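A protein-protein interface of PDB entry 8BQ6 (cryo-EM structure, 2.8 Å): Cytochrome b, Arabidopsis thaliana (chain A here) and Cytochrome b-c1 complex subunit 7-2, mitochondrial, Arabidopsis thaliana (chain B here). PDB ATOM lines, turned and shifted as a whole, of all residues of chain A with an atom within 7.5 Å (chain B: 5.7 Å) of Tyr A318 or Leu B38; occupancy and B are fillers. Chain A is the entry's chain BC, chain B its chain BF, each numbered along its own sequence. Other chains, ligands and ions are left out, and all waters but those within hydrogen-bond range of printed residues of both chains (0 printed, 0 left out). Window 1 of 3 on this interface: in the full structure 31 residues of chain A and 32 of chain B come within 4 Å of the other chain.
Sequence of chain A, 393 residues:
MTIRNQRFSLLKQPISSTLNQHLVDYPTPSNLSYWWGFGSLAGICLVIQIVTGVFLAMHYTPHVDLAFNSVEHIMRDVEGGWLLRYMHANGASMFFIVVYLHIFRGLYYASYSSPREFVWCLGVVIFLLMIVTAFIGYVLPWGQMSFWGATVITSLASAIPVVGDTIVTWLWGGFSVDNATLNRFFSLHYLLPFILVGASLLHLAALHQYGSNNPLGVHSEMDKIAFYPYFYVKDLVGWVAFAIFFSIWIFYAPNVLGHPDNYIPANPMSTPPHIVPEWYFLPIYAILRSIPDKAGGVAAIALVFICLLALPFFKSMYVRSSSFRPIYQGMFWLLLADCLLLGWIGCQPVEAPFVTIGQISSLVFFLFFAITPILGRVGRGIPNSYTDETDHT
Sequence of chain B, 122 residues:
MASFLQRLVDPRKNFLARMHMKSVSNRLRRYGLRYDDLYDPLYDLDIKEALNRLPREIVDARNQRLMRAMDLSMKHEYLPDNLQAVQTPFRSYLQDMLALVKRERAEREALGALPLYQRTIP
The guanidinium group (NH2) of Arg A320 is in salt-bridge range of the side-chain carboxylate (OD2) of Asp B40 (3.0 Å). ND1 of His A219 lies within hydrogen-bond range of OD1 of Asp B40 (3.0 Å). The side-chain hydroxyl (OG) of Ser A316 lies within hydrogen-bond range of the side-chain hydroxyl (OH) of Tyr B43. OH of Tyr A318 lies within hydrogen-bond range of NZ of Lys B102 (2.9 Å). The backbone carbonyl oxygen (O) of Met A317 sits at hydrogen-bond distance from the side-chain hydroxyl (OH) of Tyr B43 (3.0 Å). The side-chain hydroxyl (OG) of Ser A114 lies within hydrogen-bond range of the backbone carbonyl oxygen (O) of Tyr B43, at 2.8 Å.
NH2 of Arg A320 lies within hydrogen-bond range of O of Ser A114, at 3.1 Å. The backbone carbonyl oxygen (O) of Ser A316 is in hydrogen-bond range of the guanidinium group (NE) of Arg A380, at 2.6 Å. OD2 of Asp B44 is in hydrogen-bond range of N of Ile B47 (2.8 Å). N of Asp B46 sits close to OD2 of Asp B44, at 3.5 Å. The backbone carbonyl oxygen (O) of Gly A217 lies within hydrogen-bond range of the guanidinium group (NH1) of Arg A320.
Among the printed residues, pairs that only touch across the chains: Ser A113 with Tyr B43 (3.99 Å), Val A218 with Leu B38 (3.8 Å), Met A317 with Tyr B35 (3.7 Å), Tyr A318 with Leu B38 (3.8 Å), Tyr A318 with Tyr B39 (3.5 Å), Tyr A318 with Tyr B43 (3.9 Å), Tyr A318 with Asp B44 (3.4 Å), Tyr A318 with Ile B47 (3.3 Å), Val A319 with Tyr B35 (3.4 Å), Val A319 with Leu B38 (3.8 Å), Phe A324 with Leu B28 (3.9 Å), Phe A324 with Leu B38 (3.9 Å), Pro A383 with Tyr B35 (3.4 Å) and Pro A383 with Tyr B39 (3.3 Å).
Printed residues of chain B within 4 Å of Ser A114: Tyr B43 (2.8 Å). Of the printed residues of chain B, Ser A316 touches Tyr B43 (2.5 Å). Tyr A318 touches just these residues of chain B: Leu B38 (3.8 Å), Tyr B39 (3.5 Å), Tyr B43 (3.9 Å), Asp B44 (3.4 Å), Ile B47 (3.3 Å) and Lys B102 (2.9 Å). Leu B38 touches just these residues of chain A: Val A218, Tyr A318, Val A319 and Phe A324. The nearest residue of chain A that does not touch Leu B38 is Gly A217 (4.2 Å).
Of the 20 printed residues of chain A, 11 touch a printed residue of chain B. Printed residues of chain A that touch a printed residue of chain B: Ser A113, Ser A114, Val A218, His A219, Ser A316, Met A317, Tyr A318, Val A319, Arg A320, Phe A324 and Pro A383. Hydrophobic or aromatic side chains of chain A that line the printed part of chain B: Val A218, His A219, Met A317, Tyr A318, Val A319, Phe A324 and Pro A383. Along chain A the printed residues that touch a printed residue of chain B span positions 113 to 383. Of the 16 printed residues of chain B, 9 touch a printed residue of chain A. Among the printed residues, 20 pairs touch across the chains. Among the printed residues, Asp or Glu carboxylates within 4 Å of a Lys or Arg side-chain nitrogen of the other chain: Arg A320 with Asp B40 (3.0 Å).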
ATOM      1  N   SER A 113       1.384 -27.823  -5.634  1.00  0.00           N
ATOM      2  CA  SER A 113       1.722 -26.676  -4.812  1.00  0.00           C
ATOM      3  C   SER A 113       0.508 -25.774  -4.626  1.00  0.00           C
ATOM      4  O   SER A 113      -0.513 -25.903  -5.307  1.00  0.00           O
ATOM      5  CB  SER A 113       2.862 -25.880  -5.441  1.00  0.00           C
ATOM      6  OG  SER A 113       2.537 -25.519  -6.770  1.00  0.00           O
ATOM      7  N   SER A 114       0.632 -24.836  -3.686  1.00  0.00           N
ATOM      8  CA  SER A 114      -0.457 -23.862  -3.409  1.00  0.00           C
ATOM      9  C   SER A 114      -0.762 -23.032  -4.657  1.00  0.00           C
ATOM     10  O   SER A 114       0.191 -22.547  -5.284  1.00  0.00           O
ATOM     11  CB  SER A 114      -0.063 -22.999  -2.240  1.00  0.00           C
ATOM     12  OG  SER A 114      -1.004 -21.965  -2.002  1.00  0.00           O
ATOM     13  N   LEU A 216       4.347 -23.185 -17.767  1.00  0.00           N
ATOM     14  CA  LEU A 216       5.275 -22.174 -17.279  1.00  0.00           C
ATOM     15  C   LEU A 216       5.181 -21.961 -15.775  1.00  0.00           C
ATOM     16  O   LEU A 216       6.083 -21.350 -15.194  1.00  0.00           O
ATOM     17  CB  LEU A 216       5.019 -20.849 -17.988  1.00  0.00           C
ATOM     18  CG  LEU A 216       5.499 -20.759 -19.430  1.00  0.00           C
ATOM     19  CD1 LEU A 216       5.006 -19.458 -20.014  1.00  0.00           C
ATOM     20  CD2 LEU A 216       7.012 -20.862 -19.517  1.00  0.00           C
ATOM     21  N   GLY A 217       4.113 -22.442 -15.141  1.00  0.00           N
ATOM     22  CA  GLY A 217       3.936 -22.289 -13.710  1.00  0.00           C
ATOM     23  C   GLY A 217       3.702 -20.876 -13.232  1.00  0.00           C
ATOM     24  O   GLY A 217       4.046 -20.556 -12.092  1.00  0.00           O
ATOM     25  N   VAL A 218       3.110 -20.018 -14.057  1.00  0.00           N
ATOM     26  CA  VAL A 218       2.930 -18.615 -13.719  1.00  0.00           C
ATOM     27  C   VAL A 218       1.439 -18.299 -13.619  1.00  0.00           C
ATOM     28  O   VAL A 218       0.579 -19.112 -13.955  1.00  0.00           O
ATOM     29  CB  VAL A 218       3.614 -17.685 -14.737  1.00  0.00           C
ATOM     30  CG1 VAL A 218       5.104 -17.959 -14.795  1.00  0.00           C
ATOM     31  CG2 VAL A 218       2.994 -17.864 -16.092  1.00  0.00           C
ATOM     32  N   HIS A 219       1.145 -17.092 -13.138  1.00  0.00           N
ATOM     33  CA  HIS A 219      -0.213 -16.566 -13.176  1.00  0.00           C
ATOM     34  C   HIS A 219      -0.698 -16.471 -14.616  1.00  0.00           C
ATOM     35  O   HIS A 219      -0.025 -15.886 -15.468  1.00  0.00           O
ATOM     36  CB  HIS A 219      -0.252 -15.188 -12.526  1.00  0.00           C
ATOM     37  CG  HIS A 219      -1.560 -14.863 -11.881  1.00  0.00           C
ATOM     38  ND1 HIS A 219      -2.147 -15.680 -10.940  1.00  0.00           N
ATOM     39  CD2 HIS A 219      -2.408 -13.824 -12.062  1.00  0.00           C
ATOM     40  CE1 HIS A 219      -3.292 -15.149 -10.556  1.00  0.00           C
ATOM     41  NE2 HIS A 219      -3.474 -14.022 -11.220  1.00  0.00           N
ATOM     42  N   SER A 316       8.093 -24.424   0.775  1.00  0.00           N
ATOM     43  CA  SER A 316       8.834 -24.602  -0.457  1.00  0.00           C
ATOM     44  C   SER A 316       9.196 -23.246  -1.033  1.00  0.00           C
ATOM     45  O   SER A 316       8.791 -22.194  -0.525  1.00  0.00           O
ATOM     46  CB  SER A 316       8.025 -25.406  -1.478  1.00  0.00           C
ATOM     47  OG  SER A 316       7.370 -24.538  -2.388  1.00  0.00           O
ATOM     48  N   MET A 317       9.973 -23.286  -2.110  1.00  0.00           N
ATOM     49  CA  MET A 317      10.223 -22.106  -2.907  1.00  0.00           C
ATOM     50  C   MET A 317       8.968 -21.746  -3.692  1.00  0.00           C
ATOM     51  O   MET A 317       8.005 -22.511  -3.777  1.00  0.00           O
ATOM     52  CB  MET A 317      11.404 -22.327  -3.849  1.00  0.00           C
ATOM     53  CG  MET A 317      11.220 -23.470  -4.828  1.00  0.00           C
ATOM     54  SD  MET A 317      12.711 -23.773  -5.791  1.00  0.00           S
ATOM     55  CE  MET A 317      13.270 -22.098  -6.089  1.00  0.00           C
ATOM     56  N   TYR A 318       8.993 -20.558  -4.272  1.00  0.00           N
ATOM     57  CA  TYR A 318       7.814 -19.970  -4.876  1.00  0.00           C
ATOM     58  C   TYR A 318       7.727 -20.224  -6.370  1.00  0.00           C
ATOM     59  O   TYR A 318       6.753 -19.805  -7.002  1.00  0.00           O
ATOM     60  CB  TYR A 318       7.792 -18.470  -4.600  1.00  0.00           C
ATOM     61  CG  TYR A 318       7.755 -18.110  -3.131  1.00  0.00           C
ATOM     62  CD1 TYR A 318       8.795 -18.434  -2.267  1.00  0.00           C
ATOM     63  CD2 TYR A 318       6.656 -17.467  -2.607  1.00  0.00           C
ATOM     64  CE1 TYR A 318       8.733 -18.098  -0.927  1.00  0.00           C
ATOM     65  CE2 TYR A 318       6.585 -17.131  -1.287  1.00  0.00           C
ATOM     66  CZ  TYR A 318       7.616 -17.445  -0.448  1.00  0.00           C
ATOM     67  OH  TYR A 318       7.510 -17.093   0.875  1.00  0.00           O
ATOM     68  N   VAL A 319       8.702 -20.890  -6.935  1.00  0.00           N
ATOM     69  CA  VAL A 319       8.698 -21.243  -8.345  1.00  0.00           C
ATOM     70  C   VAL A 319       8.151 -22.654  -8.483  1.00  0.00           C
ATOM     71  O   VAL A 319       8.482 -23.544  -7.691  1.00  0.00           O
ATOM     72  CB  VAL A 319      10.111 -21.119  -8.937  1.00  0.00           C
ATOM     73  CG1 VAL A 319      10.107 -21.483 -10.404  1.00  0.00           C
ATOM     74  CG2 VAL A 319      10.626 -19.708  -8.731  1.00  0.00           C
ATOM     75  N   ARG A 320       7.299 -22.858  -9.486  1.00  0.00           N
ATOM     76  CA  ARG A 320       6.581 -24.113  -9.660  1.00  0.00           C
ATOM     77  C   ARG A 320       7.239 -25.026 -10.688  1.00  0.00           C
ATOM     78  O   ARG A 320       7.621 -26.155 -10.371  1.00  0.00           O
ATOM     79  CB  ARG A 320       5.136 -23.823 -10.081  1.00  0.00           C
ATOM     80  CG  ARG A 320       4.183 -23.621  -8.937  1.00  0.00           C
ATOM     81  CD  ARG A 320       2.751 -23.614  -9.424  1.00  0.00           C
ATOM     82  NE  ARG A 320       1.885 -22.844  -8.540  1.00  0.00           N
ATOM     83  CZ  ARG A 320       1.411 -21.637  -8.817  1.00  0.00           C
ATOM     84  NH1 ARG A 320       1.679 -21.036  -9.964  1.00  0.00           N
ATOM     85  NH2 ARG A 320       0.645 -21.020  -7.922  1.00  0.00           N
ATOM     86  N   SER A 321       7.384 -24.545 -11.917  1.00  0.00           N
ATOM     87  CA  SER A 321       7.693 -25.414 -13.042  1.00  0.00           C
ATOM     88  C   SER A 321       9.121 -25.939 -12.965  1.00  0.00           C
ATOM     89  O   SER A 321      10.032 -25.248 -12.502  1.00  0.00           O
ATOM     90  CB  SER A 321       7.480 -24.653 -14.349  1.00  0.00           C
ATOM     91  OG  SER A 321       7.436 -25.528 -15.459  1.00  0.00           O
ATOM     92  N   SER A 323      10.737 -26.300 -15.528  1.00  0.00           N
ATOM     93  CA  SER A 323      11.396 -25.583 -16.610  1.00  0.00           C
ATOM     94  C   SER A 323      12.290 -24.468 -16.095  1.00  0.00           C
ATOM     95  O   SER A 323      13.106 -23.939 -16.855  1.00  0.00           O
ATOM     96  CB  SER A 323      10.345 -25.011 -17.554  1.00  0.00           C
ATOM     97  OG  SER A 323       9.634 -26.056 -18.188  1.00  0.00           O
ATOM     98  N   PHE A 324      12.141 -24.088 -14.827  1.00  0.00           N
ATOM     99  CA  PHE A 324      12.972 -23.066 -14.209  1.00  0.00           C
ATOM    100  C   PHE A 324      13.620 -23.558 -12.924  1.00  0.00           C
ATOM    101  O   PHE A 324      14.245 -22.764 -12.212  1.00  0.00           O
ATOM    102  CB  PHE A 324      12.149 -21.803 -13.947  1.00  0.00           C
ATOM    103  CG  PHE A 324      11.408 -21.310 -15.154  1.00  0.00           C
ATOM    104  CD1 PHE A 324      12.089 -20.716 -16.199  1.00  0.00           C
ATOM    105  CD2 PHE A 324      10.035 -21.446 -15.249  1.00  0.00           C
ATOM    106  CE1 PHE A 324      11.419 -20.264 -17.310  1.00  0.00           C
ATOM    107  CE2 PHE A 324       9.360 -20.994 -16.360  1.00  0.00           C
ATOM    108  CZ  PHE A 324      10.052 -20.403 -17.392  1.00  0.00           C
ATOM    109  N   ARG A 325      13.496 -24.845 -12.617  1.00  0.00           N
ATOM    110  CA  ARG A 325      14.118 -25.455 -11.445  1.00  0.00           C
ATOM    111  C   ARG A 325      14.956 -26.628 -11.928  1.00  0.00           C
ATOM    112  O   ARG A 325      14.520 -27.785 -11.874  1.00  0.00           O
ATOM    113  CB  ARG A 325      13.069 -25.897 -10.425  1.00  0.00           C
ATOM    114  CG  ARG A 325      12.229 -24.763  -9.880  1.00  0.00           C
ATOM    115  CD  ARG A 325      10.933 -25.270  -9.294  1.00  0.00           C
ATOM    116  NE  ARG A 325      11.157 -25.825  -7.966  1.00  0.00           N
ATOM    117  CZ  ARG A 325      10.409 -26.767  -7.411  1.00  0.00           C
ATOM    118  NH1 ARG A 325       9.322 -27.226  -8.007  1.00  0.00           N
ATOM    119  NH2 ARG A 325      10.761 -27.259  -6.227  1.00  0.00           N
ATOM    120  N   GLY A 376      13.442 -26.357  -1.276  1.00  0.00           N
ATOM    121  CA  GLY A 376      12.668 -25.127  -1.229  1.00  0.00           C
ATOM    122  C   GLY A 376      13.230 -24.128  -0.236  1.00  0.00           C
ATOM    123  O   GLY A 376      13.277 -22.926  -0.503  1.00  0.00           O
ATOM    124  N   GLY A 379      16.168 -22.744  -1.861  1.00  0.00           N
ATOM    125  CA  GLY A 379      15.816 -21.993  -3.053  1.00  0.00           C
ATOM    126  C   GLY A 379      15.078 -20.692  -2.804  1.00  0.00           C
ATOM    127  O   GLY A 379      14.991 -19.873  -3.726  1.00  0.00           O
ATOM    128  N   ARG A 380      14.539 -20.480  -1.600  1.00  0.00           N
ATOM    129  CA  ARG A 380      13.862 -19.218  -1.320  1.00  0.00           C
ATOM    130  C   ARG A 380      14.815 -18.032  -1.339  1.00  0.00           C
ATOM    131  O   ARG A 380      14.367 -16.894  -1.513  1.00  0.00           O
ATOM    132  CB  ARG A 380      13.149 -19.274   0.031  1.00  0.00           C
ATOM    133  CG  ARG A 380      11.778 -19.912  -0.021  1.00  0.00           C
ATOM    134  CD  ARG A 380      11.313 -20.330   1.360  1.00  0.00           C
ATOM    135  NE  ARG A 380       9.929 -20.786   1.357  1.00  0.00           N
ATOM    136  CZ  ARG A 380       8.918 -20.118   1.896  1.00  0.00           C
ATOM    137  NH1 ARG A 380       9.095 -18.937   2.466  1.00  0.00           N
ATOM    138  NH2 ARG A 380       7.698 -20.649   1.863  1.00  0.00           N
ATOM    139  N   GLY A 381      16.109 -18.269  -1.151  1.00  0.00           N
ATOM    140  CA  GLY A 381      17.117 -17.235  -1.220  1.00  0.00           C
ATOM    141  C   GLY A 381      17.747 -17.031  -2.576  1.00  0.00           C
ATOM    142  O   GLY A 381      18.690 -16.244  -2.694  1.00  0.00           O
ATOM    143  N   PRO A 383      16.514 -15.472  -5.372  1.00  0.00           N
ATOM    144  CA  PRO A 383      16.424 -14.103  -5.909  1.00  0.00           C
ATOM    145  C   PRO A 383      17.395 -13.125  -5.273  1.00  0.00           C
ATOM    146  O   PRO A 383      17.918 -12.245  -5.966  1.00  0.00           O
ATOM    147  CB  PRO A 383      14.967 -13.721  -5.622  1.00  0.00           C
ATOM    148  CG  PRO A 383      14.260 -15.008  -5.583  1.00  0.00           C
ATOM    149  CD  PRO A 383      15.203 -15.921  -4.872  1.00  0.00           C
ATOM    150  N   LEU B  28      14.978 -18.256 -18.536  1.00  0.00           N
ATOM    151  CA  LEU B  28      14.080 -17.117 -18.374  1.00  0.00           C
ATOM    152  C   LEU B  28      14.172 -16.164 -19.556  1.00  0.00           C
ATOM    153  O   LEU B  28      13.179 -15.524 -19.925  1.00  0.00           O
ATOM    154  CB  LEU B  28      14.406 -16.378 -17.080  1.00  0.00           C
ATOM    155  CG  LEU B  28      13.990 -17.050 -15.775  1.00  0.00           C
ATOM    156  CD1 LEU B  28      14.751 -16.430 -14.622  1.00  0.00           C
ATOM    157  CD2 LEU B  28      12.494 -16.914 -15.572  1.00  0.00           C
ATOM    158  N   LEU B  33      10.992 -13.391 -19.520  1.00  0.00           N
ATOM    159  CA  LEU B  33      10.464 -13.363 -18.168  1.00  0.00           C
ATOM    160  C   LEU B  33      11.559 -12.953 -17.198  1.00  0.00           C
ATOM    161  O   LEU B  33      12.727 -13.309 -17.372  1.00  0.00           O
ATOM    162  CB  LEU B  33       9.912 -14.733 -17.770  1.00  0.00           C
ATOM    163  CG  LEU B  33       8.497 -15.099 -18.219  1.00  0.00           C
ATOM    164  CD1 LEU B  33       8.211 -16.553 -17.912  1.00  0.00           C
ATOM    165  CD2 LEU B  33       7.468 -14.209 -17.552  1.00  0.00           C
ATOM    166  N   ARG B  34      11.180 -12.181 -16.191  1.00  0.00           N
ATOM    167  CA  ARG B  34      12.046 -11.990 -15.044  1.00  0.00           C
ATOM    168  C   ARG B  34      11.781 -13.099 -14.040  1.00  0.00           C
ATOM    169  O   ARG B  34      10.748 -13.772 -14.079  1.00  0.00           O
ATOM    170  CB  ARG B  34      11.817 -10.625 -14.405  1.00  0.00           C
ATOM    171  CG  ARG B  34      11.709  -9.506 -15.409  1.00  0.00           C
ATOM    172  CD  ARG B  34      12.720  -8.423 -15.135  1.00  0.00           C
ATOM    173  NE  ARG B  34      12.357  -7.190 -15.819  1.00  0.00           N
ATOM    174  CZ  ARG B  34      12.342  -5.999 -15.242  1.00  0.00           C
ATOM    175  NH1 ARG B  34      12.684  -5.842 -13.974  1.00  0.00           N
ATOM    176  NH2 ARG B  34      11.959  -4.940 -15.949  1.00  0.00           N
ATOM    177  N   TYR B  35      12.746 -13.304 -13.145  1.00  0.00           N
ATOM    178  CA  TYR B  35      12.574 -14.311 -12.107  1.00  0.00           C
ATOM    179  C   TYR B  35      11.418 -13.955 -11.187  1.00  0.00           C
ATOM    180  O   TYR B  35      10.657 -14.832 -10.762  1.00  0.00           O
ATOM    181  CB  TYR B  35      13.860 -14.458 -11.304  1.00  0.00           C
ATOM    182  CG  TYR B  35      13.884 -15.696 -10.455  1.00  0.00           C
ATOM    183  CD1 TYR B  35      14.359 -16.889 -10.966  1.00  0.00           C
ATOM    184  CD2 TYR B  35      13.431 -15.674  -9.145  1.00  0.00           C
ATOM    185  CE1 TYR B  35      14.386 -18.023 -10.204  1.00  0.00           C
ATOM    186  CE2 TYR B  35      13.452 -16.809  -8.375  1.00  0.00           C
ATOM    187  CZ  TYR B  35      13.936 -17.981  -8.911  1.00  0.00           C
ATOM    188  OH  TYR B  35      13.968 -19.126  -8.155  1.00  0.00           O
ATOM    189  N   ASP B  36      11.279 -12.673 -10.856  1.00  0.00           N
ATOM    190  CA  ASP B  36      10.189 -12.242  -9.995  1.00  0.00           C
ATOM    191  C   ASP B  36       8.827 -12.492 -10.624  1.00  0.00           C
ATOM    192  O   ASP B  36       7.833 -12.568  -9.897  1.00  0.00           O
ATOM    193  CB  ASP B  36      10.346 -10.762  -9.654  1.00  0.00           C
ATOM    194  CG  ASP B  36      11.371 -10.519  -8.564  1.00  0.00           C
ATOM    195  OD1 ASP B  36      11.827 -11.495  -7.933  1.00  0.00           O
ATOM    196  OD2 ASP B  36      11.725  -9.347  -8.339  1.00  0.00           O
ATOM    197  N   ASP B  37       8.759 -12.625 -11.952  1.00  0.00           N
ATOM    198  CA  ASP B  37       7.489 -12.934 -12.596  1.00  0.00           C
ATOM    199  C   ASP B  37       7.003 -14.337 -12.281  1.00  0.00           C
ATOM    200  O   ASP B  37       5.809 -14.612 -12.437  1.00  0.00           O
ATOM    201  CB  ASP B  37       7.589 -12.772 -14.110  1.00  0.00           C
ATOM    202  CG  ASP B  37       7.937 -11.369 -14.520  1.00  0.00           C
ATOM    203  OD1 ASP B  37       7.784 -10.455 -13.690  1.00  0.00           O
ATOM    204  OD2 ASP B  37       8.340 -11.172 -15.681  1.00  0.00           O
ATOM    205  N   LEU B  38       7.895 -15.235 -11.859  1.00  0.00           N
ATOM    206  CA  LEU B  38       7.480 -16.578 -11.481  1.00  0.00           C
ATOM    207  C   LEU B  38       6.716 -16.608 -10.168  1.00  0.00           C
ATOM    208  O   LEU B  38       5.973 -17.564  -9.921  1.00  0.00           O
ATOM    209  CB  LEU B  38       8.695 -17.499 -11.389  1.00  0.00           C
ATOM    210  CG  LEU B  38       9.579 -17.504 -12.634  1.00  0.00           C
ATOM    211  CD1 LEU B  38      10.859 -18.276 -12.383  1.00  0.00           C
ATOM    212  CD2 LEU B  38       8.812 -18.082 -13.803  1.00  0.00           C
ATOM    213  N   TYR B  39       6.879 -15.594  -9.325  1.00  0.00           N
ATOM    214  CA  TYR B  39       6.157 -15.516  -8.060  1.00  0.00           C
ATOM    215  C   TYR B  39       4.698 -15.181  -8.349  1.00  0.00           C
ATOM    216  O   TYR B  39       4.401 -14.161  -8.977  1.00  0.00           O
ATOM    217  CB  TYR B  39       6.800 -14.465  -7.162  1.00  0.00           C
ATOM    218  CG  TYR B  39       8.038 -14.939  -6.436  1.00  0.00           C
ATOM    219  CD1 TYR B  39       9.091 -15.522  -7.125  1.00  0.00           C
ATOM    220  CD2 TYR B  39       8.162 -14.781  -5.066  1.00  0.00           C
ATOM    221  CE1 TYR B  39      10.222 -15.947  -6.471  1.00  0.00           C
ATOM    222  CE2 TYR B  39       9.294 -15.202  -4.402  1.00  0.00           C
ATOM    223  CZ  TYR B  39      10.319 -15.785  -5.111  1.00  0.00           C
ATOM    224  OH  TYR B  39      11.449 -16.211  -4.458  1.00  0.00           O
ATOM    225  N   ASP B  40       3.791 -16.038  -7.896  1.00  0.00           N
ATOM    226  CA  ASP B  40       2.358 -16.025  -8.180  1.00  0.00           C
ATOM    227  C   ASP B  40       1.601 -15.409  -7.005  1.00  0.00           C
ATOM    228  O   ASP B  40       1.871 -15.768  -5.855  1.00  0.00           O
ATOM    229  CB  ASP B  40       1.870 -17.454  -8.439  1.00  0.00           C
ATOM    230  CG  ASP B  40       0.422 -17.519  -8.909  1.00  0.00           C
ATOM    231  OD1 ASP B  40      -0.333 -16.568  -8.673  1.00  0.00           O
ATOM    232  OD2 ASP B  40       0.020 -18.537  -9.518  1.00  0.00           O
ATOM    233  N   TYR B  43      -0.012 -18.150  -5.030  1.00  0.00           N
ATOM    234  CA  TYR B  43       0.834 -19.022  -4.228  1.00  0.00           C
ATOM    235  C   TYR B  43       0.705 -18.697  -2.745  1.00  0.00           C
ATOM    236  O   TYR B  43       0.543 -19.599  -1.916  1.00  0.00           O
ATOM    237  CB  TYR B  43       2.286 -18.926  -4.683  1.00  0.00           C
ATOM    238  CG  TYR B  43       3.123 -20.040  -4.123  1.00  0.00           C
ATOM    239  CD1 TYR B  43       3.667 -19.955  -2.853  1.00  0.00           C
ATOM    240  CD2 TYR B  43       3.319 -21.204  -4.842  1.00  0.00           C
ATOM    241  CE1 TYR B  43       4.415 -20.984  -2.331  1.00  0.00           C
ATOM    242  CE2 TYR B  43       4.060 -22.236  -4.329  1.00  0.00           C
ATOM    243  CZ  TYR B  43       4.608 -22.123  -3.074  1.00  0.00           C
ATOM    244  OH  TYR B  43       5.353 -23.157  -2.564  1.00  0.00           O
ATOM    245  N   ASP B  44       0.771 -17.420  -2.386  1.00  0.00           N
ATOM    246  CA  ASP B  44       0.511 -17.044  -1.005  1.00  0.00           C
ATOM    247  C   ASP B  44      -0.080 -15.645  -0.956  1.00  0.00           C
ATOM    248  O   ASP B  44       0.063 -14.855  -1.893  1.00  0.00           O
ATOM    249  CB  ASP B  44       1.772 -17.152  -0.129  1.00  0.00           C
ATOM    250  CG  ASP B  44       2.802 -16.089  -0.438  1.00  0.00           C
ATOM    251  OD1 ASP B  44       3.810 -16.006   0.293  1.00  0.00           O
ATOM    252  OD2 ASP B  44       2.638 -15.361  -1.428  1.00  0.00           O
ATOM    253  N   ASP B  46       0.945 -13.304   0.822  1.00  0.00           N
ATOM    254  CA  ASP B  46       1.998 -12.299   0.963  1.00  0.00           C
ATOM    255  C   ASP B  46       2.401 -11.713  -0.382  1.00  0.00           C
ATOM    256  O   ASP B  46       2.602 -10.498  -0.497  1.00  0.00           O
ATOM    257  CB  ASP B  46       3.214 -12.901   1.658  1.00  0.00           C
ATOM    258  CG  ASP B  46       2.898 -13.389   3.044  1.00  0.00           C
ATOM    259  OD1 ASP B  46       2.170 -12.677   3.767  1.00  0.00           O
ATOM    260  OD2 ASP B  46       3.369 -14.485   3.407  1.00  0.00           O
ATOM    261  N   ILE B  47       2.548 -12.558  -1.405  1.00  0.00           N
ATOM    262  CA  ILE B  47       2.867 -12.057  -2.739  1.00  0.00           C
ATOM    263  C   ILE B  47       1.748 -11.158  -3.238  1.00  0.00           C
ATOM    264  O   ILE B  47       1.995 -10.117  -3.858  1.00  0.00           O
ATOM    265  CB  ILE B  47       3.128 -13.226  -3.707  1.00  0.00           C
ATOM    266  CG1 ILE B  47       4.472 -13.883  -3.408  1.00  0.00           C
ATOM    267  CG2 ILE B  47       3.114 -12.751  -5.143  1.00  0.00           C
ATOM    268  CD1 ILE B  47       4.604 -15.241  -4.027  1.00  0.00           C
ATOM    269  N   ARG B  62       4.631  -6.350 -15.664  1.00  0.00           N
ATOM    270  CA  ARG B  62       4.700  -7.760 -15.300  1.00  0.00           C
ATOM    271  C   ARG B  62       3.586  -8.553 -15.973  1.00  0.00           C
ATOM    272  O   ARG B  62       3.804  -9.679 -16.436  1.00  0.00           O
ATOM    273  CB  ARG B  62       4.637  -7.912 -13.782  1.00  0.00           C
ATOM    274  CG  ARG B  62       4.085  -9.240 -13.334  1.00  0.00           C
ATOM    275  CD  ARG B  62       3.681  -9.212 -11.881  1.00  0.00           C
ATOM    276  NE  ARG B  62       3.039 -10.460 -11.491  1.00  0.00           N
ATOM    277  CZ  ARG B  62       3.658 -11.472 -10.901  1.00  0.00           C
ATOM    278  NH1 ARG B  62       4.943 -11.412 -10.593  1.00  0.00           N
ATOM    279  NH2 ARG B  62       2.971 -12.573 -10.613  1.00  0.00           N
ATOM    280  N   LEU B  98       8.368  -7.790  -0.885  1.00  0.00           N
ATOM    281  CA  LEU B  98       7.928  -9.005  -0.208  1.00  0.00           C
ATOM    282  C   LEU B  98       8.596  -9.157   1.154  1.00  0.00           C
ATOM    283  O   LEU B  98       7.954  -9.572   2.125  1.00  0.00           O
ATOM    284  CB  LEU B  98       8.213 -10.216  -1.095  1.00  0.00           C
ATOM    285  CG  LEU B  98       7.775 -11.609  -0.640  1.00  0.00           C
ATOM    286  CD1 LEU B  98       6.290 -11.671  -0.335  1.00  0.00           C
ATOM    287  CD2 LEU B  98       8.141 -12.630  -1.697  1.00  0.00           C
ATOM    288  N   LYS B 102       6.716  -9.350   4.788  1.00  0.00           N
ATOM    289  CA  LYS B 102       6.953 -10.415   5.757  1.00  0.00           C
ATOM    290  C   LYS B 102       7.372  -9.853   7.109  1.00  0.00           C
ATOM    291  O   LYS B 102       7.017 -10.405   8.155  1.00  0.00           O
ATOM    292  CB  LYS B 102       8.013 -11.384   5.234  1.00  0.00           C
ATOM    293  CG  LYS B 102       7.659 -12.094   3.939  1.00  0.00           C
ATOM    294  CD  LYS B 102       8.892 -12.783   3.369  1.00  0.00           C
ATOM    295  CE  LYS B 102       8.562 -13.646   2.163  1.00  0.00           C
ATOM    296  NZ  LYS B 102       7.485 -14.628   2.451  1.00  0.00           N
